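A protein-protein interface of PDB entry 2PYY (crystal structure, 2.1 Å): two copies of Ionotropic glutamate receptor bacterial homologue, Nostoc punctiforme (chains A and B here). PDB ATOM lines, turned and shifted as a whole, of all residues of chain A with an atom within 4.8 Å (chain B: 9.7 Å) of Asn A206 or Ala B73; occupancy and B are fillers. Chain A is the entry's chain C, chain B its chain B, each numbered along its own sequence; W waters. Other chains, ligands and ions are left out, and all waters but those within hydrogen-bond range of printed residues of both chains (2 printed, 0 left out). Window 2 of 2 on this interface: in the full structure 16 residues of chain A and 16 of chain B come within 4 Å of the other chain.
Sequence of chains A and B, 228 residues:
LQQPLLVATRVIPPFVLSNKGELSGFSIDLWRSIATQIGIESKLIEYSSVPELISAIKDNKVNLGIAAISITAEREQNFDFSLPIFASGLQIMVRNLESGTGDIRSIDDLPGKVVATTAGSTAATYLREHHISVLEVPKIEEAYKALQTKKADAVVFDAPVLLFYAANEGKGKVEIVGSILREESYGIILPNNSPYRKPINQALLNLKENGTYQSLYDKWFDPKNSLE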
ATOM      1  N   GLN A  37      28.403   3.817 -21.829  1.00  0.00           N
ATOM      2  CA  GLN A  37      28.336   3.306 -20.465  1.00  0.00           C
ATOM      3  C   GLN A  37      28.315   1.785 -20.474  1.00  0.00           C
ATOM      4  O   GLN A  37      28.943   1.133 -19.641  1.00  0.00           O
ATOM      5  CB  GLN A  37      27.071   3.824 -19.780  1.00  0.00           C
ATOM      6  CG  GLN A  37      27.331   4.776 -18.637  1.00  0.00           C
ATOM      7  CD  GLN A  37      28.173   4.140 -17.547  1.00  0.00           C
ATOM      8  OE1 GLN A  37      27.879   3.038 -17.080  1.00  0.00           O
ATOM      9  NE2 GLN A  37      29.225   4.836 -17.133  1.00  0.00           N
ATOM     10  N   GLN A 202      20.613   0.247 -15.939  1.00  0.00           N
ATOM     11  CA  GLN A 202      21.843   0.255 -15.159  1.00  0.00           C
ATOM     12  C   GLN A 202      22.709   1.463 -15.546  1.00  0.00           C
ATOM     13  O   GLN A 202      23.135   2.223 -14.686  1.00  0.00           O
ATOM     14  CB  GLN A 202      22.601  -1.045 -15.434  1.00  0.00           C
ATOM     15  CG  GLN A 202      23.903  -1.214 -14.693  1.00  0.00           C
ATOM     16  CD  GLN A 202      23.711  -1.299 -13.200  1.00  0.00           C
ATOM     17  OE1 GLN A 202      22.705  -1.832 -12.726  1.00  0.00           O
ATOM     18  NE2 GLN A 202      24.681  -0.788 -12.446  1.00  0.00           N
ATOM     19  N   ALA A 203      22.950   1.636 -16.844  1.00  0.00           N
ATOM     20  CA  ALA A 203      23.764   2.744 -17.347  1.00  0.00           C
ATOM     21  C   ALA A 203      23.137   4.088 -17.002  1.00  0.00           C
ATOM     22  O   ALA A 203      23.803   5.017 -16.538  1.00  0.00           O
ATOM     23  CB  ALA A 203      23.922   2.630 -18.858  1.00  0.00           C
ATOM     24  N   LEU A 204      21.841   4.181 -17.255  1.00  0.00           N
ATOM     25  CA  LEU A 204      21.101   5.396 -16.983  1.00  0.00           C
ATOM     26  C   LEU A 204      21.232   5.748 -15.506  1.00  0.00           C
ATOM     27  O   LEU A 204      21.483   6.900 -15.156  1.00  0.00           O
ATOM     28  CB  LEU A 204      19.635   5.193 -17.349  1.00  0.00           C
ATOM     29  CG  LEU A 204      18.721   6.399 -17.173  1.00  0.00           C
ATOM     30  CD1 LEU A 204      19.149   7.525 -18.111  1.00  0.00           C
ATOM     31  CD2 LEU A 204      17.292   5.972 -17.466  1.00  0.00           C
ATOM     32  N   LEU A 205      21.068   4.758 -14.633  1.00  0.00           N
ATOM     33  CA  LEU A 205      21.195   5.036 -13.210  1.00  0.00           C
ATOM     34  C   LEU A 205      22.608   5.557 -12.900  1.00  0.00           C
ATOM     35  O   LEU A 205      22.759   6.519 -12.146  1.00  0.00           O
ATOM     36  CB  LEU A 205      20.833   3.792 -12.375  1.00  0.00           C
ATOM     37  CG  LEU A 205      19.319   3.513 -12.428  1.00  0.00           C
ATOM     38  CD1 LEU A 205      19.035   2.056 -12.194  1.00  0.00           C
ATOM     39  CD2 LEU A 205      18.585   4.388 -11.410  1.00  0.00           C
ATOM     40  N   ASN A 206      23.633   4.950 -13.496  1.00  0.00           N
ATOM     41  CA  ASN A 206      25.009   5.403 -13.280  1.00  0.00           C
ATOM     42  C   ASN A 206      25.145   6.871 -13.656  1.00  0.00           C
ATOM     43  O   ASN A 206      25.684   7.674 -12.896  1.00  0.00           O
ATOM     44  CB  ASN A 206      25.995   4.595 -14.132  1.00  0.00           C
ATOM     45  CG  ASN A 206      26.153   3.165 -13.645  1.00  0.00           C
ATOM     46  OD1 ASN A 206      26.289   2.922 -12.440  1.00  0.00           O
ATOM     47  ND2 ASN A 206      26.156   2.216 -14.575  1.00  0.00           N
ATOM     48  N   LEU A 207      24.649   7.217 -14.842  1.00  0.00           N
ATOM     49  CA  LEU A 207      24.718   8.584 -15.333  1.00  0.00           C
ATOM     50  C   LEU A 207      24.041   9.541 -14.371  1.00  0.00           C
ATOM     51  O   LEU A 207      24.490  10.668 -14.186  1.00  0.00           O
ATOM     52  CB  LEU A 207      24.059   8.686 -16.714  1.00  0.00           C
ATOM     53  CG  LEU A 207      24.677   7.830 -17.817  1.00  0.00           C
ATOM     54  CD1 LEU A 207      23.917   8.049 -19.116  1.00  0.00           C
ATOM     55  CD2 LEU A 207      26.146   8.198 -18.004  1.00  0.00           C
ATOM     56  N   LYS A 208      22.945   9.098 -13.772  1.00  0.00           N
ATOM     57  CA  LYS A 208      22.228   9.934 -12.822  1.00  0.00           C
ATOM     58  C   LYS A 208      22.981   9.985 -11.497  1.00  0.00           C
ATOM     59  O   LYS A 208      22.931  10.984 -10.783  1.00  0.00           O
ATOM     60  CB  LYS A 208      20.821   9.385 -12.592  1.00  0.00           C
ATOM     61  CG  LYS A 208      19.858   9.638 -13.738  1.00  0.00           C
ATOM     62  CD  LYS A 208      18.628   8.770 -13.607  1.00  0.00           C
ATOM     63  CE  LYS A 208      17.626   9.066 -14.702  1.00  0.00           C
ATOM     64  NZ  LYS A 208      17.051  10.429 -14.553  1.00  0.00           N
ATOM     65  N   GLU A 209      23.678   8.899 -11.175  1.00  0.00           N
ATOM     66  CA  GLU A 209      24.436   8.818  -9.931  1.00  0.00           C
ATOM     67  C   GLU A 209      25.836   9.449  -9.994  1.00  0.00           C
ATOM     68  O   GLU A 209      26.401   9.801  -8.958  1.00  0.00           O
ATOM     69  CB  GLU A 209      24.541   7.359  -9.480  1.00  0.00           C
ATOM     70  CG  GLU A 209      23.280   6.815  -8.815  1.00  0.00           C
ATOM     71  CD  GLU A 209      23.299   5.291  -8.650  1.00  0.00           C
ATOM     72  OE1 GLU A 209      24.373   4.732  -8.329  1.00  0.00           O
ATOM     73  OE2 GLU A 209      22.231   4.654  -8.833  1.00  0.00           O
ATOM     74  N   ASN A 210      26.400   9.598 -11.188  1.00  0.00           N
ATOM     75  CA  ASN A 210      27.728  10.199 -11.289  1.00  0.00           C
ATOM     76  C   ASN A 210      27.672  11.658 -11.731  1.00  0.00           C
ATOM     77  O   ASN A 210      28.703  12.319 -11.835  1.00  0.00           O
ATOM     78  CB  ASN A 210      28.622   9.412 -12.253  1.00  0.00           C
ATOM     79  CG  ASN A 210      28.139   9.489 -13.676  1.00  0.00           C
ATOM     80  OD1 ASN A 210      27.624  10.517 -14.111  1.00  0.00           O
ATOM     81  ND2 ASN A 210      28.311   8.407 -14.417  1.00  0.00           N
ATOM     82  N   GLY A 211      26.470  12.155 -12.005  1.00  0.00           N
ATOM     83  CA  GLY A 211      26.329  13.546 -12.405  1.00  0.00           C
ATOM     84  C   GLY A 211      26.268  13.875 -13.888  1.00  0.00           C
ATOM     85  O   GLY A 211      26.133  15.043 -14.252  1.00  0.00           O
ATOM     86  N   SER B  70      14.607   3.387  -2.774  1.00  0.00           N
ATOM     87  CA  SER B  70      15.307   4.075  -3.850  1.00  0.00           C
ATOM     88  C   SER B  70      15.802   3.114  -4.919  1.00  0.00           C
ATOM     89  O   SER B  70      16.344   2.051  -4.620  1.00  0.00           O
ATOM     90  CB  SER B  70      16.499   4.837  -3.280  1.00  0.00           C
ATOM     91  OG  SER B  70      16.059   5.817  -2.367  1.00  0.00           O
ATOM     92  N   ILE B  71      15.606   3.505  -6.170  1.00  0.00           N
ATOM     93  CA  ILE B  71      16.064   2.734  -7.311  1.00  0.00           C
ATOM     94  C   ILE B  71      17.510   3.192  -7.554  1.00  0.00           C
ATOM     95  O   ILE B  71      17.777   4.388  -7.736  1.00  0.00           O
ATOM     96  CB  ILE B  71      15.206   3.056  -8.558  1.00  0.00           C
ATOM     97  CG1 ILE B  71      13.742   2.672  -8.275  1.00  0.00           C
ATOM     98  CG2 ILE B  71      15.743   2.309  -9.796  1.00  0.00           C
ATOM     99  CD1 ILE B  71      12.799   2.981  -9.401  1.00  0.00           C
ATOM    100  N   THR B  72      18.447   2.253  -7.547  1.00  0.00           N
ATOM    101  CA  THR B  72      19.845   2.594  -7.767  1.00  0.00           C
ATOM    102  C   THR B  72      20.480   1.625  -8.732  1.00  0.00           C
ATOM    103  O   THR B  72      19.936   0.557  -9.009  1.00  0.00           O
ATOM    104  CB  THR B  72      20.666   2.541  -6.467  1.00  0.00           C
ATOM    105  OG1 THR B  72      20.687   1.200  -5.975  1.00  0.00           O
ATOM    106  CG2 THR B  72      20.060   3.448  -5.411  1.00  0.00           C
ATOM    107  N   ALA B  73      21.652   1.994  -9.233  1.00  0.00           N
ATOM    108  CA  ALA B  73      22.370   1.146 -10.172  1.00  0.00           C
ATOM    109  C   ALA B  73      22.736  -0.194  -9.547  1.00  0.00           C
ATOM    110  O   ALA B  73      22.594  -1.248 -10.173  1.00  0.00           O
ATOM    111  CB  ALA B  73      23.639   1.855 -10.656  1.00  0.00           C
ATOM    112  N   GLU B  74      23.205  -0.148  -8.307  1.00  0.00           N
ATOM    113  CA  GLU B  74      23.622  -1.351  -7.592  1.00  0.00           C
ATOM    114  C   GLU B  74      22.478  -2.335  -7.359  1.00  0.00           C
ATOM    115  O   GLU B  74      22.636  -3.550  -7.510  1.00  0.00           O
ATOM    116  CB  GLU B  74      24.233  -0.957  -6.250  1.00  0.00           C
ATOM    117  CG  GLU B  74      24.509  -2.120  -5.328  1.00  0.00           C
ATOM    118  CD  GLU B  74      24.929  -1.647  -3.962  1.00  0.00           C
ATOM    119  OE1 GLU B  74      24.199  -0.812  -3.371  1.00  0.00           O
ATOM    120  OE2 GLU B  74      25.988  -2.102  -3.477  1.00  0.00           O
ATOM    121  N   ARG B  75      21.330  -1.800  -6.960  1.00  0.00           N
ATOM    122  CA  ARG B  75      20.161  -2.627  -6.721  1.00  0.00           C
ATOM    123  C   ARG B  75      19.600  -3.151  -8.045  1.00  0.00           C
ATOM    124  O   ARG B  75      19.155  -4.297  -8.139  1.00  0.00           O
ATOM    125  CB  ARG B  75      19.097  -1.823  -5.959  1.00  0.00           C
ATOM    126  CG  ARG B  75      19.567  -1.413  -4.564  1.00  0.00           C
ATOM    127  CD  ARG B  75      18.584  -0.497  -3.853  1.00  0.00           C
ATOM    128  NE  ARG B  75      19.013  -0.218  -2.486  1.00  0.00           N
ATOM    129  CZ  ARG B  75      18.431   0.660  -1.679  1.00  0.00           C
ATOM    130  NH1 ARG B  75      17.378   1.367  -2.098  1.00  0.00           N
ATOM    131  NH2 ARG B  75      18.907   0.825  -0.451  1.00  0.00           N
ATOM    132  N   GLU B  76      19.646  -2.314  -9.072  1.00  0.00           N
ATOM    133  CA  GLU B  76      19.142  -2.693 -10.383  1.00  0.00           C
ATOM    134  C   GLU B  76      19.969  -3.817 -10.998  1.00  0.00           C
ATOM    135  O   GLU B  76      19.487  -4.572 -11.845  1.00  0.00           O
ATOM    136  CB  GLU B  76      19.154  -1.480 -11.305  1.00  0.00           C
ATOM    137  CG  GLU B  76      17.964  -1.408 -12.254  1.00  0.00           C
ATOM    138  CD  GLU B  76      18.005  -2.470 -13.323  1.00  0.00           C
ATOM    139  OE1 GLU B  76      19.093  -2.661 -13.911  1.00  0.00           O
ATOM    140  OE2 GLU B  76      16.952  -3.103 -13.589  1.00  0.00           O
ATOM    141  N   GLN B  77      21.214  -3.935 -10.562  1.00  0.00           N
ATOM    142  CA  GLN B  77      22.082  -4.965 -11.094  1.00  0.00           C
ATOM    143  C   GLN B  77      21.605  -6.372 -10.750  1.00  0.00           C
ATOM    144  O   GLN B  77      21.657  -7.281 -11.581  1.00  0.00           O
ATOM    145  CB  GLN B  77      23.502  -4.766 -10.578  1.00  0.00           C
ATOM    146  CG  GLN B  77      24.503  -5.736 -11.181  1.00  0.00           C
ATOM    147  CD  GLN B  77      25.905  -5.489 -10.672  1.00  0.00           C
ATOM    148  OE1 GLN B  77      26.515  -4.458 -10.974  1.00  0.00           O
ATOM    149  NE2 GLN B  77      26.425  -6.431  -9.886  1.00  0.00           N
ATOM    150  N   ASN B  78      21.117  -6.551  -9.530  1.00  0.00           N
ATOM    151  CA  ASN B  78      20.662  -7.868  -9.094  1.00  0.00           C
ATOM    152  C   ASN B  78      19.167  -8.018  -8.914  1.00  0.00           C
ATOM    153  O   ASN B  78      18.666  -9.127  -8.697  1.00  0.00           O
ATOM    154  CB  ASN B  78      21.374  -8.239  -7.800  1.00  0.00           C
ATOM    155  CG  ASN B  78      22.868  -8.322  -7.984  1.00  0.00           C
ATOM    156  OD1 ASN B  78      23.366  -9.235  -8.635  1.00  0.00           O
ATOM    157  ND2 ASN B  78      23.590  -7.361  -7.429  1.00  0.00           N
ATOM    158  N   PHE B  79      18.451  -6.905  -9.007  1.00  0.00           N
ATOM    159  CA  PHE B  79      17.006  -6.935  -8.835  1.00  0.00           C
ATOM    160  C   PHE B  79      16.296  -6.105  -9.897  1.00  0.00           C
ATOM    161  O   PHE B  79      16.930  -5.368 -10.643  1.00  0.00           O
ATOM    162  CB  PHE B  79      16.647  -6.448  -7.424  1.00  0.00           C
ATOM    163  CG  PHE B  79      17.319  -7.237  -6.329  1.00  0.00           C
ATOM    164  CD1 PHE B  79      18.596  -6.893  -5.885  1.00  0.00           C
ATOM    165  CD2 PHE B  79      16.710  -8.374  -5.803  1.00  0.00           C
ATOM    166  CE1 PHE B  79      19.259  -7.676  -4.940  1.00  0.00           C
ATOM    167  CE2 PHE B  79      17.361  -9.162  -4.861  1.00  0.00           C
ATOM    168  CZ  PHE B  79      18.641  -8.813  -4.430  1.00  0.00           C
ATOM    169  N   ASP B  80      14.981  -6.261  -9.980  1.00  0.00           N
ATOM    170  CA  ASP B  80      14.192  -5.535 -10.964  1.00  0.00           C
ATOM    171  C   ASP B  80      13.322  -4.490 -10.254  1.00  0.00           C
ATOM    172  O   ASP B  80      12.996  -4.639  -9.076  1.00  0.00           O
ATOM    173  CB  ASP B  80      13.303  -6.506 -11.744  1.00  0.00           C
ATOM    174  CG  ASP B  80      13.470  -6.372 -13.248  1.00  0.00           C
ATOM    175  OD1 ASP B  80      13.973  -5.320 -13.692  1.00  0.00           O
ATOM    176  OD2 ASP B  80      13.078  -7.307 -13.980  1.00  0.00           O
ATOM    177  N   PHE B  81      12.956  -3.441 -10.980  1.00  0.00           N
ATOM    178  CA  PHE B  81      12.125  -2.384 -10.438  1.00  0.00           C
ATOM    179  C   PHE B  81      10.967  -2.063 -11.376  1.00  0.00           C
ATOM    180  O   PHE B  81      11.086  -2.211 -12.588  1.00  0.00           O
ATOM    181  CB  PHE B  81      12.936  -1.100 -10.234  1.00  0.00           C
ATOM    182  CG  PHE B  81      13.722  -1.063  -8.956  1.00  0.00           C
ATOM    183  CD1 PHE B  81      15.081  -1.344  -8.954  1.00  0.00           C
ATOM    184  CD2 PHE B  81      13.102  -0.751  -7.754  1.00  0.00           C
ATOM    185  CE1 PHE B  81      15.817  -1.316  -7.766  1.00  0.00           C
ATOM    186  CE2 PHE B  81      13.826  -0.720  -6.560  1.00  0.00           C
ATOM    187  CZ  PHE B  81      15.184  -1.005  -6.569  1.00  0.00           C
ATOM    188  N   THR B 122      20.465   4.610   1.174  1.00  0.00           N
ATOM    189  CA  THR B 122      21.175   5.279   0.095  1.00  0.00           C
ATOM    190  C   THR B 122      21.904   6.488   0.686  1.00  0.00           C
ATOM    191  O   THR B 122      22.912   6.938   0.143  1.00  0.00           O
ATOM    192  CB  THR B 122      20.220   5.740  -1.035  1.00  0.00           C
ATOM    193  OG1 THR B 122      19.213   6.606  -0.496  1.00  0.00           O
ATOM    194  CG2 THR B 122      19.555   4.532  -1.696  1.00  0.00           C
ATOM    195  N   THR B 125      25.286   5.350   2.076  1.00  0.00           N
ATOM    196  CA  THR B 125      26.154   5.103   0.929  1.00  0.00           C
ATOM    197  C   THR B 125      26.713   6.436   0.411  1.00  0.00           C
ATOM    198  O   THR B 125      27.927   6.603   0.254  1.00  0.00           O
ATOM    199  CB  THR B 125      25.381   4.382  -0.213  1.00  0.00           C
ATOM    200  OG1 THR B 125      25.023   3.071   0.225  1.00  0.00           O
ATOM    201  CG2 THR B 125      26.236   4.254  -1.474  1.00  0.00           C
ATOM    202  N   GLU B 129      30.733   7.357   0.545  1.00  0.00           N
ATOM    203  CA  GLU B 129      31.401   7.619  -0.719  1.00  0.00           C
ATOM    204  C   GLU B 129      31.953   9.040  -0.819  1.00  0.00           C
ATOM    205  O   GLU B 129      32.931   9.276  -1.526  1.00  0.00           O
ATOM    206  CB  GLU B 129      30.449   7.331  -1.878  1.00  0.00           C
ATOM    207  CG  GLU B 129      30.168   5.846  -2.070  1.00  0.00           C
ATOM    208  CD  GLU B 129      29.105   5.586  -3.124  1.00  0.00           C
ATOM    209  OE1 GLU B 129      28.935   4.413  -3.527  1.00  0.00           O
ATOM    210  OE2 GLU B 129      28.438   6.567  -3.541  1.00  0.00           O
ATOM    211  N   ARG B 182      20.946  14.729  -3.785  1.00  0.00           N
ATOM    212  CA  ARG B 182      20.894  13.807  -4.906  1.00  0.00           C
ATOM    213  C   ARG B 182      19.441  13.362  -5.076  1.00  0.00           C
ATOM    214  O   ARG B 182      18.752  13.051  -4.098  1.00  0.00           O
ATOM    215  CB  ARG B 182      21.795  12.580  -4.665  1.00  0.00           C
ATOM    216  CG  ARG B 182      21.876  11.643  -5.883  1.00  0.00           C
ATOM    217  CD  ARG B 182      22.968  10.558  -5.804  1.00  0.00           C
ATOM    218  NE  ARG B 182      22.645   9.452  -4.892  1.00  0.00           N
ATOM    219  CZ  ARG B 182      23.335   8.310  -4.806  1.00  0.00           C
ATOM    220  NH1 ARG B 182      24.396   8.106  -5.576  1.00  0.00           N
ATOM    221  NH2 ARG B 182      22.968   7.371  -3.938  1.00  0.00           N
ATOM    222  N   GLU B 183      18.977  13.350  -6.320  1.00  0.00           N
ATOM    223  CA  GLU B 183      17.616  12.941  -6.619  1.00  0.00           C
ATOM    224  C   GLU B 183      17.505  11.448  -6.825  1.00  0.00           C
ATOM    225  O   GLU B 183      18.274  10.853  -7.582  1.00  0.00           O
ATOM    226  CB  GLU B 183      17.107  13.645  -7.872  1.00  0.00           C
ATOM    227  CG  GLU B 183      16.771  15.105  -7.665  1.00  0.00           C
ATOM    228  CD  GLU B 183      16.282  15.777  -8.931  1.00  0.00           C
ATOM    229  OE1 GLU B 183      15.765  16.913  -8.828  1.00  0.00           O
ATOM    230  OE2 GLU B 183      16.417  15.176 -10.028  1.00  0.00           O
ATOM    231  N   GLU B 184      16.537  10.842  -6.152  1.00  0.00           N
ATOM    232  CA  GLU B 184      16.313   9.407  -6.277  1.00  0.00           C
ATOM    233  C   GLU B 184      14.820   9.185  -6.434  1.00  0.00           C
ATOM    234  O   GLU B 184      14.013   9.953  -5.920  1.00  0.00           O
ATOM    235  CB  GLU B 184      16.784   8.667  -5.017  1.00  0.00           C
ATOM    236  CG  GLU B 184      18.173   9.045  -4.509  1.00  0.00           C
ATOM    237  CD  GLU B 184      18.681   8.126  -3.401  1.00  0.00           C
ATOM    238  OE1 GLU B 184      17.940   7.885  -2.405  1.00  0.00           O
ATOM    239  OE2 GLU B 184      19.840   7.658  -3.523  1.00  0.00           O
ATOM    240  N   SER B 185      14.446   8.146  -7.157  1.00  0.00           N
ATOM    241  CA  SER B 185      13.038   7.862  -7.305  1.00  0.00           C
ATOM    242  C   SER B 185      12.806   6.543  -6.578  1.00  0.00           C
ATOM    243  O   SER B 185      13.737   5.740  -6.407  1.00  0.00           O
ATOM    244  CB  SER B 185      12.652   7.763  -8.787  1.00  0.00           C
ATOM    245  OG  SER B 185      12.963   6.492  -9.319  1.00  0.00           O
HETATM  246  O   HOH W   1      19.996   6.193  -8.170  1.00  0.00           O
HETATM  247  O   HOH W   2      24.325   2.207  -7.311  1.00  0.00           O
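The backbone carbonyl oxygen (O) of Ala B73 lies close to the side-chain amide oxygen (OE1) of Gln A202. The side-chain carboxylate of Glu A209 is in hydrogen-bond range of the backbone NH of Ala B73 (2.8 Å). OE1 of Gln A202 sits at hydrogen-bond distance from N of Gln B77, at 3.4 Å.
O of Ser B185 is in hydrogen-bond range of N of Ile B71 (2.9 Å). The side-chain hydroxyl (OG1) of Thr B72 sits close to the backbone NH (N) of Arg B75, 3.2 Å away. The guanidinium group of Arg B182 is in salt-bridge range of the side-chain carboxylate of Glu B184 (3.2 Å). OE1 of Gln A37 is in hydrogen-bond range of ND2 of Asn A206 (3.1 Å). ND2 of Asn A206 is in hydrogen-bond range of O of Gln A202 (3.0 Å). The backbone carbonyl oxygen (O) of Asn A206 lies within hydrogen-bond range of the side-chain amide nitrogen (ND2) of Asn A210 (3.1 Å).
Among the printed residues, pairs that only touch across the chains: Glu A209 with Thr B72 (3.3 Å), Asn A206 with Ala B73 (3.4 Å), Leu A205 with Glu B76 (3.6 Å), Leu A205 with Thr B72 (3.6 Å), Glu A209 with Arg B182 (3.7 Å), Leu A205 with Ala B73 (3.7 Å), Leu A205 with Ile B71 (3.8 Å) and Gln A202 with Glu B76 (3.8 Å).
Of chain B, only Ala B73 (3.4 Å) comes within 4 Å of Asn A206. Of chain A, only Gln A202 (2.6 Å), Leu A205 (3.7 Å), Asn A206 (3.4 Å) and Glu A209 (2.8 Å) come within 4 Å of Ala B73. Glu A209 touches three residues of chain B. No residue of chain B comes within 4 Å of Asn A210. Of the printed residues of chain B, Gln A202 touches Ala B73, Glu B76 and Gln B77. Of the printed residues of chain A, Gln B77 touches Gln A202 (3.4 Å). Thr B122 touches none of the printed residues of chain A. Ser B185 touches none of the printed residues of chain A. The nearest printed residue of chain A that does not touch Ala B73 is Ala A203 (6.2 Å). The nearest printed residue of chain A that does not touch Ile B71 is Glu A209 (4.6 Å).
Printed residues of chain B that touch a printed residue of chain A: Ile B71, Thr B72, Ala B73, Glu B76, Gln B77 and Arg B182. Hydrophobic or aromatic side chains of chain B that line the printed part of chain A: Ile B71 and Ala B73. Of the 11 printed residues of chain A, 4 touch a printed residue of chain B. Hydrophobic or aromatic side chains of chain A within 4 Å of the printed part of chain B: Leu A205. Among the printed residues, 11 pairs touch across the chains. Among the printed residues, no Asp or Glu carboxylate lies within 4 Å of a Lys or Arg side-chain nitrogen of the other chain.
No position is printed for both chains.
Water W2 lies within hydrogen-bond range of OE1 of Glu A209 (2.7 Å), N of Glu B74 (2.8 Å) and N of Ala B73 (3.3 Å). Water W1 bridges OE2 of Glu A209 (2.8 Å) and O of Ile B71 (2.9 Å).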
